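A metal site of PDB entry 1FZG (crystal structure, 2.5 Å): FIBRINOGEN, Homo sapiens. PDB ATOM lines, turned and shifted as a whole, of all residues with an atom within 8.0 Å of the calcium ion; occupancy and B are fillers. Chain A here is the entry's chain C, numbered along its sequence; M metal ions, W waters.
Of the 14 residues printed, 4 come within 4 Å of the calcium ion.
OD2 of Asp 233 sits at hydrogen-bond distance from N of Cys 239 (2.9 Å). The backbone NH of Asp 233 is in hydrogen-bond range of the side-chain hydroxyl of Ser 226, at 3.3 Å.
The calcium ion is bound by O of Gly 237 (2.2 Å). OD1 of Asp 233 binds the calcium ion (2.2 Å). The calcium ion is bound by water W1. OD1 of Asp 231 is bound to the calcium ion, at 2.4 Å. The backbone carbonyl oxygen (O) of Phe 235 binds the calcium ion, at 2.4 Å. OD2 of Asp 231 is bound to the calcium ion.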
ATOM      1  N   SER A 226      16.259  19.683  18.037  1.00  0.00           N
ATOM      2  CA  SER A 226      15.585  18.743  17.110  1.00  0.00           C
ATOM      3  C   SER A 226      16.632  17.835  16.524  1.00  0.00           C
ATOM      4  O   SER A 226      17.790  18.208  16.434  1.00  0.00           O
ATOM      5  CB  SER A 226      14.910  19.499  15.986  1.00  0.00           C
ATOM      6  OG  SER A 226      13.809  20.265  16.442  1.00  0.00           O
ATOM      7  N   ASN A 230      12.979  13.586  15.608  1.00  0.00           N
ATOM      8  CA  ASN A 230      12.141  14.151  16.713  1.00  0.00           C
ATOM      9  C   ASN A 230      12.119  15.650  16.429  1.00  0.00           C
ATOM     10  O   ASN A 230      13.008  16.358  16.864  1.00  0.00           O
ATOM     11  CB  ASN A 230      12.719  13.683  18.018  1.00  0.00           C
ATOM     12  CG  ASN A 230      11.926  14.136  19.221  1.00  0.00           C
ATOM     13  OD1 ASN A 230      11.783  13.336  20.152  1.00  0.00           O
ATOM     14  ND2 ASN A 230      11.431  15.349  19.295  1.00  0.00           N
ATOM     15  N   ASP A 231      11.199  16.079  15.563  1.00  0.00           N
ATOM     16  CA  ASP A 231      11.197  17.422  14.995  1.00  0.00           C
ATOM     17  C   ASP A 231      10.519  18.394  15.960  1.00  0.00           C
ATOM     18  O   ASP A 231       9.369  18.096  16.204  1.00  0.00           O
ATOM     19  CB  ASP A 231      10.527  17.455  13.665  1.00  0.00           C
ATOM     20  CG  ASP A 231      10.400  18.606  12.753  1.00  0.00           C
ATOM     21  OD1 ASP A 231      10.443  19.760  13.214  1.00  0.00           O
ATOM     22  OD2 ASP A 231      10.271  18.431  11.509  1.00  0.00           O
ATOM     23  N   ASN A 232      11.251  19.432  16.364  1.00  0.00           N
ATOM     24  CA  ASN A 232      10.553  20.350  17.248  1.00  0.00           C
ATOM     25  C   ASN A 232      10.826  21.757  16.709  1.00  0.00           C
ATOM     26  O   ASN A 232      10.806  22.698  17.525  1.00  0.00           O
ATOM     27  CB  ASN A 232      11.029  20.248  18.708  1.00  0.00           C
ATOM     28  CG  ASN A 232      10.923  18.800  19.198  1.00  0.00           C
ATOM     29  OD1 ASN A 232      11.935  18.100  19.438  1.00  0.00           O
ATOM     30  ND2 ASN A 232       9.734  18.282  19.388  1.00  0.00           N
ATOM     31  N   ASP A 233      11.102  21.836  15.390  1.00  0.00           N
ATOM     32  CA  ASP A 233      11.494  23.169  14.900  1.00  0.00           C
ATOM     33  C   ASP A 233      10.386  24.137  14.545  1.00  0.00           C
ATOM     34  O   ASP A 233       9.214  23.833  14.843  1.00  0.00           O
ATOM     35  CB  ASP A 233      12.455  22.905  13.759  1.00  0.00           C
ATOM     36  CG  ASP A 233      11.815  22.347  12.519  1.00  0.00           C
ATOM     37  OD1 ASP A 233      10.568  22.231  12.432  1.00  0.00           O
ATOM     38  OD2 ASP A 233      12.635  22.070  11.603  1.00  0.00           O
ATOM     39  N   LYS A 234      10.673  25.296  13.922  1.00  0.00           N
ATOM     40  CA  LYS A 234       9.562  26.228  13.586  1.00  0.00           C
ATOM     41  C   LYS A 234       9.406  26.270  12.072  1.00  0.00           C
ATOM     42  O   LYS A 234       9.296  27.352  11.530  1.00  0.00           O
ATOM     43  CB  LYS A 234       9.749  27.690  14.027  1.00  0.00           C
ATOM     44  CG  LYS A 234       9.975  27.871  15.509  1.00  0.00           C
ATOM     45  CD  LYS A 234       8.933  27.103  16.313  1.00  0.00           C
ATOM     46  CE  LYS A 234       8.970  27.521  17.776  1.00  0.00           C
ATOM     47  NZ  LYS A 234       7.670  27.354  18.487  1.00  0.00           N
ATOM     48  N   PHE A 235       9.500  25.115  11.477  1.00  0.00           N
ATOM     49  CA  PHE A 235       9.446  24.953  10.019  1.00  0.00           C
ATOM     50  C   PHE A 235       8.454  23.811   9.794  1.00  0.00           C
ATOM     51  O   PHE A 235       8.307  22.882  10.587  1.00  0.00           O
ATOM     52  CB  PHE A 235      10.853  24.623   9.542  1.00  0.00           C
ATOM     53  CG  PHE A 235      11.106  24.241   8.125  1.00  0.00           C
ATOM     54  CD1 PHE A 235      10.350  24.817   7.097  1.00  0.00           C
ATOM     55  CD2 PHE A 235      12.071  23.338   7.756  1.00  0.00           C
ATOM     56  CE1 PHE A 235      10.546  24.542   5.776  1.00  0.00           C
ATOM     57  CE2 PHE A 235      12.341  23.042   6.421  1.00  0.00           C
ATOM     58  CZ  PHE A 235      11.556  23.652   5.460  1.00  0.00           C
ATOM     59  N   GLU A 236       7.698  23.926   8.755  1.00  0.00           N
ATOM     60  CA  GLU A 236       6.643  22.986   8.357  1.00  0.00           C
ATOM     61  C   GLU A 236       7.391  21.755   7.897  1.00  0.00           C
ATOM     62  O   GLU A 236       6.875  20.657   7.881  1.00  0.00           O
ATOM     63  CB  GLU A 236       5.755  23.574   7.291  1.00  0.00           C
ATOM     64  CG  GLU A 236       6.409  24.582   6.337  1.00  0.00           C
ATOM     65  CD  GLU A 236       6.835  25.906   6.997  1.00  0.00           C
ATOM     66  OE1 GLU A 236       6.353  26.232   8.114  1.00  0.00           O
ATOM     67  OE2 GLU A 236       7.671  26.594   6.365  1.00  0.00           O
ATOM     68  N   GLY A 237       8.669  21.921   7.575  1.00  0.00           N
ATOM     69  CA  GLY A 237       9.472  20.731   7.249  1.00  0.00           C
ATOM     70  C   GLY A 237      10.310  20.354   8.486  1.00  0.00           C
ATOM     71  O   GLY A 237      10.117  20.717   9.639  1.00  0.00           O
ATOM     72  N   ASN A 238      11.345  19.576   8.161  1.00  0.00           N
ATOM     73  CA  ASN A 238      12.290  19.026   9.119  1.00  0.00           C
ATOM     74  C   ASN A 238      13.747  19.512   8.915  1.00  0.00           C
ATOM     75  O   ASN A 238      14.530  18.815   8.249  1.00  0.00           O
ATOM     76  CB  ASN A 238      12.265  17.502   9.065  1.00  0.00           C
ATOM     77  CG  ASN A 238      12.962  16.928  10.315  1.00  0.00           C
ATOM     78  OD1 ASN A 238      12.609  15.798  10.728  1.00  0.00           O
ATOM     79  ND2 ASN A 238      13.895  17.631  10.966  1.00  0.00           N
ATOM     80  N   CYS A 239      14.037  20.636   9.536  1.00  0.00           N
ATOM     81  CA  CYS A 239      15.348  21.268   9.403  1.00  0.00           C
ATOM     82  C   CYS A 239      16.517  20.321   9.627  1.00  0.00           C
ATOM     83  O   CYS A 239      17.516  20.245   8.904  1.00  0.00           O
ATOM     84  CB  CYS A 239      15.409  22.417  10.448  1.00  0.00           C
ATOM     85  SG  CYS A 239      14.491  23.958  10.159  1.00  0.00           S
ATOM     86  N   ALA A 240      16.548  19.587  10.745  1.00  0.00           N
ATOM     87  CA  ALA A 240      17.571  18.690  11.198  1.00  0.00           C
ATOM     88  C   ALA A 240      17.792  17.549  10.219  1.00  0.00           C
ATOM     89  O   ALA A 240      18.952  17.210  10.005  1.00  0.00           O
ATOM     90  CB  ALA A 240      17.286  18.124  12.598  1.00  0.00           C
ATOM     91  N   MET A 249      17.088  24.140  16.317  1.00  0.00           N
ATOM     92  CA  MET A 249      16.702  24.619  14.992  1.00  0.00           C
ATOM     93  C   MET A 249      15.552  25.601  15.019  1.00  0.00           C
ATOM     94  O   MET A 249      14.611  25.324  15.778  1.00  0.00           O
ATOM     95  CB  MET A 249      16.199  23.427  14.138  1.00  0.00           C
ATOM     96  CG  MET A 249      17.357  22.481  13.745  1.00  0.00           C
ATOM     97  SD  MET A 249      18.613  23.340  12.870  1.00  0.00           S
ATOM     98  CE  MET A 249      19.743  22.151  12.187  1.00  0.00           C
ATOM     99  N   LYS A 251      13.545  26.973  11.746  1.00  0.00           N
ATOM    100  CA  LYS A 251      13.443  27.509  10.347  1.00  0.00           C
ATOM    101  C   LYS A 251      14.495  28.374   9.697  1.00  0.00           C
ATOM    102  O   LYS A 251      14.118  29.334   8.990  1.00  0.00           O
ATOM    103  CB  LYS A 251      12.112  28.248  10.261  1.00  0.00           C
ATOM    104  CG  LYS A 251      11.529  28.574   8.930  1.00  0.00           C
ATOM    105  CD  LYS A 251      10.089  29.038   8.982  1.00  0.00           C
ATOM    106  CE  LYS A 251       9.488  29.210   7.576  1.00  0.00           C
ATOM    107  NZ  LYS A 251       7.991  29.365   7.704  1.00  0.00           N
HETATM  108 CA    CA M   1       9.124  20.854  11.550  1.00  0.00          CA
HETATM  109  O   HOH W   1       8.405  21.886  13.447  1.00  0.00           O
